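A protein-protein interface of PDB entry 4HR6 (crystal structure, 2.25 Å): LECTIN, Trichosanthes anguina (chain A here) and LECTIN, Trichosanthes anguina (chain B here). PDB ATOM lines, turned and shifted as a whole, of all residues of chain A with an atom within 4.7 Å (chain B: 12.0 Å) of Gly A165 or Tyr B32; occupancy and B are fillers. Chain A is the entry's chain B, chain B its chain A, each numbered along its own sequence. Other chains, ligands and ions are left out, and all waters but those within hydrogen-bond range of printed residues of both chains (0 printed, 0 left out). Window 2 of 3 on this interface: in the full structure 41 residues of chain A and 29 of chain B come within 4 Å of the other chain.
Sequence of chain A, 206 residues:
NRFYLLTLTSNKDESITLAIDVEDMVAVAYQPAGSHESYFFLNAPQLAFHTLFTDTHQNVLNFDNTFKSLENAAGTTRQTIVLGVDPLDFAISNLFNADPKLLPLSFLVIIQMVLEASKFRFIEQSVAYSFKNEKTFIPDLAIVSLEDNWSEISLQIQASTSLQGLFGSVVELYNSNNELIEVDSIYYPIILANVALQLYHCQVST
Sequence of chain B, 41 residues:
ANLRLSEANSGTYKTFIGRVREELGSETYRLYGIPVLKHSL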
ATOM      1  N   ILE A 157     -21.187 -22.051  18.272  1.00  0.00           N
ATOM      2  CA  ILE A 157     -22.153 -21.228  17.557  1.00  0.00           C
ATOM      3  C   ILE A 157     -23.479 -21.209  18.304  1.00  0.00           C
ATOM      4  O   ILE A 157     -24.080 -20.144  18.501  1.00  0.00           O
ATOM      5  CB  ILE A 157     -22.380 -21.716  16.112  1.00  0.00           C
ATOM      6  CG1 ILE A 157     -21.138 -21.433  15.284  1.00  0.00           C
ATOM      7  CG2 ILE A 157     -23.582 -21.012  15.472  1.00  0.00           C
ATOM      8  CD1 ILE A 157     -21.186 -22.021  13.890  1.00  0.00           C
ATOM      9  N   SER A 160     -23.188 -19.334  21.571  1.00  0.00           N
ATOM     10  CA  SER A 160     -23.025 -17.897  21.365  1.00  0.00           C
ATOM     11  C   SER A 160     -24.329 -17.120  21.338  1.00  0.00           C
ATOM     12  O   SER A 160     -24.321 -15.910  21.532  1.00  0.00           O
ATOM     13  CB  SER A 160     -22.294 -17.631  20.053  1.00  0.00           C
ATOM     14  OG  SER A 160     -23.207 -17.730  18.960  1.00  0.00           O
ATOM     15  N   THR A 161     -25.446 -17.797  21.095  1.00  0.00           N
ATOM     16  CA  THR A 161     -26.722 -17.113  21.050  1.00  0.00           C
ATOM     17  C   THR A 161     -27.154 -16.567  22.409  1.00  0.00           C
ATOM     18  O   THR A 161     -28.045 -15.723  22.463  1.00  0.00           O
ATOM     19  CB  THR A 161     -27.851 -18.021  20.561  1.00  0.00           C
ATOM     20  OG1 THR A 161     -27.957 -19.155  21.421  1.00  0.00           O
ATOM     21  CG2 THR A 161     -27.595 -18.473  19.132  1.00  0.00           C
ATOM     22  N   LEU A 163     -25.007 -15.049  24.561  1.00  0.00           N
ATOM     23  CA  LEU A 163     -24.187 -13.914  24.959  1.00  0.00           C
ATOM     24  C   LEU A 163     -23.540 -13.171  23.779  1.00  0.00           C
ATOM     25  O   LEU A 163     -22.320 -13.158  23.642  1.00  0.00           O
ATOM     26  CB  LEU A 163     -23.110 -14.367  25.948  1.00  0.00           C
ATOM     27  CG  LEU A 163     -22.477 -13.201  26.737  1.00  0.00           C
ATOM     28  CD1 LEU A 163     -23.427 -12.706  27.818  1.00  0.00           C
ATOM     29  CD2 LEU A 163     -21.154 -13.588  27.355  1.00  0.00           C
ATOM     30  N   GLN A 164     -24.358 -12.550  22.933  1.00  0.00           N
ATOM     31  CA  GLN A 164     -23.860 -11.536  21.988  1.00  0.00           C
ATOM     32  C   GLN A 164     -22.895 -12.099  20.934  1.00  0.00           C
ATOM     33  O   GLN A 164     -22.024 -11.381  20.461  1.00  0.00           O
ATOM     34  CB  GLN A 164     -23.115 -10.415  22.754  1.00  0.00           C
ATOM     35  CG  GLN A 164     -23.895  -9.739  23.874  1.00  0.00           C
ATOM     36  CD  GLN A 164     -24.683  -8.532  23.393  1.00  0.00           C
ATOM     37  OE1 GLN A 164     -25.118  -8.466  22.238  1.00  0.00           O
ATOM     38  NE2 GLN A 164     -24.862  -7.562  24.282  1.00  0.00           N
ATOM     39  N   GLY A 165     -23.014 -13.383  20.608  1.00  0.00           N
ATOM     40  CA  GLY A 165     -22.167 -13.988  19.576  1.00  0.00           C
ATOM     41  C   GLY A 165     -20.793 -14.393  20.057  1.00  0.00           C
ATOM     42  O   GLY A 165     -19.943 -14.783  19.260  1.00  0.00           O
ATOM     43  N   LEU A 166     -20.579 -14.329  21.367  1.00  0.00           N
ATOM     44  CA  LEU A 166     -19.329 -14.756  21.952  1.00  0.00           C
ATOM     45  C   LEU A 166     -19.357 -16.242  22.304  1.00  0.00           C
ATOM     46  O   LEU A 166     -20.348 -16.765  22.820  1.00  0.00           O
ATOM     47  CB  LEU A 166     -19.026 -13.937  23.211  1.00  0.00           C
ATOM     48  CG  LEU A 166     -18.634 -12.480  22.900  1.00  0.00           C
ATOM     49  CD1 LEU A 166     -19.108 -11.533  23.990  1.00  0.00           C
ATOM     50  CD2 LEU A 166     -17.134 -12.363  22.710  1.00  0.00           C
ATOM     51  N   PHE A 167     -18.238 -16.900  22.045  1.00  0.00           N
ATOM     52  CA  PHE A 167     -18.074 -18.309  22.334  1.00  0.00           C
ATOM     53  C   PHE A 167     -17.854 -18.518  23.833  1.00  0.00           C
ATOM     54  O   PHE A 167     -17.418 -17.613  24.538  1.00  0.00           O
ATOM     55  CB  PHE A 167     -16.858 -18.846  21.570  1.00  0.00           C
ATOM     56  CG  PHE A 167     -17.071 -19.001  20.085  1.00  0.00           C
ATOM     57  CD1 PHE A 167     -16.090 -19.594  19.319  1.00  0.00           C
ATOM     58  CD2 PHE A 167     -18.255 -18.617  19.469  1.00  0.00           C
ATOM     59  CE1 PHE A 167     -16.254 -19.781  17.959  1.00  0.00           C
ATOM     60  CE2 PHE A 167     -18.432 -18.808  18.112  1.00  0.00           C
ATOM     61  CZ  PHE A 167     -17.430 -19.395  17.359  1.00  0.00           C
ATOM     62  N   SER A 185     -15.437 -15.863  18.999  1.00  0.00           N
ATOM     63  CA  SER A 185     -16.742 -15.280  18.697  1.00  0.00           C
ATOM     64  C   SER A 185     -17.141 -15.623  17.280  1.00  0.00           C
ATOM     65  O   SER A 185     -16.336 -16.113  16.508  1.00  0.00           O
ATOM     66  CB  SER A 185     -16.709 -13.749  18.850  1.00  0.00           C
ATOM     67  OG  SER A 185     -15.999 -13.156  17.779  1.00  0.00           O
ATOM     68  N   ILE A 186     -18.382 -15.340  16.930  1.00  0.00           N
ATOM     69  CA  ILE A 186     -18.827 -15.543  15.564  1.00  0.00           C
ATOM     70  C   ILE A 186     -18.374 -14.463  14.572  1.00  0.00           C
ATOM     71  O   ILE A 186     -18.591 -14.617  13.383  1.00  0.00           O
ATOM     72  CB  ILE A 186     -20.346 -15.572  15.461  1.00  0.00           C
ATOM     73  CG1 ILE A 186     -20.933 -14.315  16.100  1.00  0.00           C
ATOM     74  CG2 ILE A 186     -20.888 -16.849  16.071  1.00  0.00           C
ATOM     75  CD1 ILE A 186     -22.208 -13.884  15.434  1.00  0.00           C
ATOM     76  N   TYR A 187     -17.758 -13.381  15.054  1.00  0.00           N
ATOM     77  CA  TYR A 187     -17.533 -12.197  14.228  1.00  0.00           C
ATOM     78  C   TYR A 187     -16.258 -12.354  13.430  1.00  0.00           C
ATOM     79  O   TYR A 187     -15.501 -11.404  13.289  1.00  0.00           O
ATOM     80  CB  TYR A 187     -17.506 -10.926  15.106  1.00  0.00           C
ATOM     81  CG  TYR A 187     -18.781 -10.790  15.884  1.00  0.00           C
ATOM     82  CD1 TYR A 187     -18.809 -10.959  17.259  1.00  0.00           C
ATOM     83  CD2 TYR A 187     -19.965 -10.577  15.236  1.00  0.00           C
ATOM     84  CE1 TYR A 187     -19.988 -10.867  17.972  1.00  0.00           C
ATOM     85  CE2 TYR A 187     -21.153 -10.495  15.934  1.00  0.00           C
ATOM     86  CZ  TYR A 187     -21.144 -10.633  17.304  1.00  0.00           C
ATOM     87  OH  TYR A 187     -22.325 -10.553  17.983  1.00  0.00           O
ATOM     88  N   LEU A 192     -18.231 -17.637  10.171  1.00  0.00           N
ATOM     89  CA  LEU A 192     -19.542 -17.305   9.681  1.00  0.00           C
ATOM     90  C   LEU A 192     -19.723 -17.574   8.187  1.00  0.00           C
ATOM     91  O   LEU A 192     -20.796 -17.978   7.761  1.00  0.00           O
ATOM     92  CB  LEU A 192     -19.816 -15.821   9.972  1.00  0.00           C
ATOM     93  CG  LEU A 192     -21.260 -15.376   9.753  1.00  0.00           C
ATOM     94  CD1 LEU A 192     -22.175 -16.195  10.648  1.00  0.00           C
ATOM     95  CD2 LEU A 192     -21.441 -13.888  10.015  1.00  0.00           C
ATOM     96  N   THR A 206     -31.856 -17.621  17.579  1.00  0.00           N
ATOM     97  CA  THR A 206     -31.805 -16.188  17.262  1.00  0.00           C
ATOM     98  C   THR A 206     -33.049 -15.861  16.441  1.00  0.00           C
ATOM     99  O   THR A 206     -33.363 -14.698  16.202  1.00  0.00           O
ATOM    100  CB  THR A 206     -30.556 -15.786  16.438  1.00  0.00           C
ATOM    101  OG1 THR A 206     -30.436 -16.617  15.273  1.00  0.00           O
ATOM    102  CG2 THR A 206     -29.289 -15.902  17.267  1.00  0.00           C
ATOM    103  N   SER B  26     -31.346 -28.153   7.684  1.00  0.00           N
ATOM    104  CA  SER B  26     -32.714 -27.769   8.007  1.00  0.00           C
ATOM    105  C   SER B  26     -33.111 -26.534   7.216  1.00  0.00           C
ATOM    106  O   SER B  26     -32.337 -25.575   7.114  1.00  0.00           O
ATOM    107  CB  SER B  26     -32.856 -27.467   9.502  1.00  0.00           C
ATOM    108  OG  SER B  26     -34.154 -26.965   9.813  1.00  0.00           O
ATOM    109  N   GLU B  27     -34.321 -26.571   6.660  1.00  0.00           N
ATOM    110  CA  GLU B  27     -34.901 -25.404   6.000  1.00  0.00           C
ATOM    111  C   GLU B  27     -35.266 -24.330   7.025  1.00  0.00           C
ATOM    112  O   GLU B  27     -35.149 -23.148   6.736  1.00  0.00           O
ATOM    113  CB  GLU B  27     -36.144 -25.786   5.173  1.00  0.00           C
ATOM    114  CG  GLU B  27     -35.847 -26.427   3.811  1.00  0.00           C
ATOM    115  CD  GLU B  27     -36.231 -27.900   3.722  1.00  0.00           C
ATOM    116  OE1 GLU B  27     -35.416 -28.704   3.213  1.00  0.00           O
ATOM    117  OE2 GLU B  27     -37.354 -28.256   4.144  1.00  0.00           O
ATOM    118  N   THR B  28     -35.665 -24.741   8.227  1.00  0.00           N
ATOM    119  CA  THR B  28     -36.221 -23.811   9.217  1.00  0.00           C
ATOM    120  C   THR B  28     -35.278 -23.437  10.384  1.00  0.00           C
ATOM    121  O   THR B  28     -35.273 -22.283  10.824  1.00  0.00           O
ATOM    122  CB  THR B  28     -37.542 -24.365   9.782  1.00  0.00           C
ATOM    123  OG1 THR B  28     -37.297 -25.598  10.468  1.00  0.00           O
ATOM    124  CG2 THR B  28     -38.541 -24.615   8.650  1.00  0.00           C
ATOM    125  N   TYR B  29     -34.481 -24.391  10.875  1.00  0.00           N
ATOM    126  CA  TYR B  29     -33.632 -24.152  12.041  1.00  0.00           C
ATOM    127  C   TYR B  29     -32.218 -23.724  11.626  1.00  0.00           C
ATOM    128  O   TYR B  29     -31.373 -24.556  11.287  1.00  0.00           O
ATOM    129  CB  TYR B  29     -33.632 -25.386  12.956  1.00  0.00           C
ATOM    130  CG  TYR B  29     -32.952 -25.215  14.301  1.00  0.00           C
ATOM    131  CD1 TYR B  29     -32.722 -23.956  14.861  1.00  0.00           C
ATOM    132  CD2 TYR B  29     -32.561 -26.325  15.032  1.00  0.00           C
ATOM    133  CE1 TYR B  29     -32.096 -23.825  16.093  1.00  0.00           C
ATOM    134  CE2 TYR B  29     -31.933 -26.204  16.261  1.00  0.00           C
ATOM    135  CZ  TYR B  29     -31.707 -24.960  16.794  1.00  0.00           C
ATOM    136  OH  TYR B  29     -31.070 -24.855  18.013  1.00  0.00           O
ATOM    137  N   ARG B  30     -31.989 -22.409  11.667  1.00  0.00           N
ATOM    138  CA  ARG B  30     -30.748 -21.772  11.243  1.00  0.00           C
ATOM    139  C   ARG B  30     -30.321 -20.745  12.266  1.00  0.00           C
ATOM    140  O   ARG B  30     -31.153 -20.068  12.848  1.00  0.00           O
ATOM    141  CB  ARG B  30     -30.942 -21.049   9.905  1.00  0.00           C
ATOM    142  CG  ARG B  30     -31.087 -21.955   8.697  1.00  0.00           C
ATOM    143  CD  ARG B  30     -31.573 -21.188   7.477  1.00  0.00           C
ATOM    144  NE  ARG B  30     -32.009 -22.100   6.417  1.00  0.00           N
ATOM    145  CZ  ARG B  30     -31.345 -22.352   5.285  1.00  0.00           C
ATOM    146  NH1 ARG B  30     -30.183 -21.757   5.019  1.00  0.00           N
ATOM    147  NH2 ARG B  30     -31.853 -23.211   4.406  1.00  0.00           N
ATOM    148  N   LEU B  31     -29.018 -20.604  12.468  1.00  0.00           N
ATOM    149  CA  LEU B  31     -28.500 -19.639  13.416  1.00  0.00           C
ATOM    150  C   LEU B  31     -27.470 -18.801  12.687  1.00  0.00           C
ATOM    151  O   LEU B  31     -26.508 -19.329  12.144  1.00  0.00           O
ATOM    152  CB  LEU B  31     -27.852 -20.347  14.613  1.00  0.00           C
ATOM    153  CG  LEU B  31     -28.728 -21.280  15.477  1.00  0.00           C
ATOM    154  CD1 LEU B  31     -27.855 -22.000  16.503  1.00  0.00           C
ATOM    155  CD2 LEU B  31     -29.866 -20.540  16.182  1.00  0.00           C
ATOM    156  N   TYR B  32     -27.671 -17.492  12.696  1.00  0.00           N
ATOM    157  CA  TYR B  32     -26.881 -16.578  11.903  1.00  0.00           C
ATOM    158  C   TYR B  32     -26.862 -16.997  10.407  1.00  0.00           C
ATOM    159  O   TYR B  32     -25.883 -16.769   9.721  1.00  0.00           O
ATOM    160  CB  TYR B  32     -25.460 -16.493  12.449  1.00  0.00           C
ATOM    161  CG  TYR B  32     -25.311 -16.303  13.951  1.00  0.00           C
ATOM    162  CD1 TYR B  32     -24.933 -17.373  14.776  1.00  0.00           C
ATOM    163  CD2 TYR B  32     -25.506 -15.057  14.547  1.00  0.00           C
ATOM    164  CE1 TYR B  32     -24.776 -17.211  16.142  1.00  0.00           C
ATOM    165  CE2 TYR B  32     -25.349 -14.880  15.923  1.00  0.00           C
ATOM    166  CZ  TYR B  32     -24.981 -15.960  16.719  1.00  0.00           C
ATOM    167  OH  TYR B  32     -24.813 -15.800  18.088  1.00  0.00           O
ATOM    168  N   GLY B  33     -27.928 -17.634   9.932  1.00  0.00           N
ATOM    169  CA  GLY B  33     -28.009 -18.148   8.548  1.00  0.00           C
ATOM    170  C   GLY B  33     -27.403 -19.532   8.265  1.00  0.00           C
ATOM    171  O   GLY B  33     -27.539 -20.057   7.157  1.00  0.00           O
ATOM    172  N   ILE B  34     -26.722 -20.118   9.252  1.00  0.00           N
ATOM    173  CA  ILE B  34     -26.086 -21.428   9.088  1.00  0.00           C
ATOM    174  C   ILE B  34     -27.047 -22.531   9.526  1.00  0.00           C
ATOM    175  O   ILE B  34     -27.456 -22.564  10.670  1.00  0.00           O
ATOM    176  CB  ILE B  34     -24.813 -21.521   9.928  1.00  0.00           C
ATOM    177  CG1 ILE B  34     -23.894 -20.349   9.598  1.00  0.00           C
ATOM    178  CG2 ILE B  34     -24.113 -22.854   9.693  1.00  0.00           C
ATOM    179  CD1 ILE B  34     -22.682 -20.250  10.497  1.00  0.00           C
ATOM    180  N   PRO B  35     -27.425 -23.430   8.615  1.00  0.00           N
ATOM    181  CA  PRO B  35     -28.384 -24.463   8.997  1.00  0.00           C
ATOM    182  C   PRO B  35     -27.849 -25.536   9.966  1.00  0.00           C
ATOM    183  O   PRO B  35     -26.709 -25.975   9.857  1.00  0.00           O
ATOM    184  CB  PRO B  35     -28.784 -25.104   7.667  1.00  0.00           C
ATOM    185  CG  PRO B  35     -27.934 -24.504   6.603  1.00  0.00           C
ATOM    186  CD  PRO B  35     -26.982 -23.540   7.213  1.00  0.00           C
ATOM    187  N   VAL B  36     -28.699 -25.940  10.899  1.00  0.00           N
ATOM    188  CA  VAL B  36     -28.461 -27.097  11.732  1.00  0.00           C
ATOM    189  C   VAL B  36     -28.919 -28.307  10.943  1.00  0.00           C
ATOM    190  O   VAL B  36     -29.858 -28.199  10.176  1.00  0.00           O
ATOM    191  CB  VAL B  36     -29.268 -27.028  13.040  1.00  0.00           C
ATOM    192  CG1 VAL B  36     -28.910 -28.210  13.941  1.00  0.00           C
ATOM    193  CG2 VAL B  36     -29.016 -25.705  13.757  1.00  0.00           C
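Among the printed residues, pairs that only touch across the chains: Ile A186 with Tyr B32 (3.3 Å), Gly A165 with Tyr B32 (3.5 Å), Thr A161 with Tyr B32 (3.7 Å), Leu A192 with Tyr B32 (3.8 Å), Thr A206 with Leu B31 (3.8 Å), Ile A157 with Tyr B32 (3.8 Å) and Thr A206 with Tyr B32 (3.9 Å).
Of the 13 printed residues of chain A, 7 touch a printed residue of chain B.
Hydrophobic or aromatic side chains of chain A that line the printed part of chain B: Ile A157, Ile A186 and Leu A192.
Printed residues of chain B that touch a printed residue of chain A: Leu B31 and Tyr B32.
Hydrophobic or aromatic side chains of chain B that line the printed part of chain A: Leu B31 and Tyr B32.
N of Gly A165 sits at hydrogen-bond distance from O of Ser A160 (3.0 Å).
The backbone carbonyl oxygen (O) of Ile A157 is in hydrogen-bond range of the side-chain hydroxyl (OG) of Ser A160 (2.6 Å).
The backbone NH (N) of Ile A186 is in hydrogen-bond range of the backbone carbonyl oxygen (O) of Gly A165 (2.9 Å).
Of chain B, only Tyr B32 (3.7 Å) comes within 4 Å of Thr A161.
No residue of chain B comes within 4 Å of Leu A163.
No residue of chain B comes within 4 Å of Gln A164.
Gly A165 touches just one residue of chain B: Tyr B32 (3.5 Å).
No residue of chain B comes within 4 Å of Leu A166.
No residue of chain B comes within 4 Å of Ser A185.
Printed residues of chain B within 4 Å of Ile A186: Tyr B32 (3.3 Å).
Printed residues of chain B within 4 Å of Thr A206: Leu B31 and Tyr B32.
Tyr B29 touches none of the printed residues of chain A.
Of the printed residues of chain A, Leu B31 touches Thr A206.
Of chain A, only Ile A157, Ser A160, Thr A161, Gly A165, Ile A186, Leu A192 and Thr A206 come within 4 Å of Tyr B32.
The nearest residue of chain B that does not touch Gly A165 is Leu B31 (9.9 Å).
The nearest printed residue of chain A that does not touch Tyr B32 is Gln A164 (5.0 Å).
The nearest printed residue of chain A that does not touch Leu B31 is Thr A161 (4.3 Å).
The side-chain hydroxyl of Tyr B32 is in hydrogen-bond range of the side-chain hydroxyl of Ser A160.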
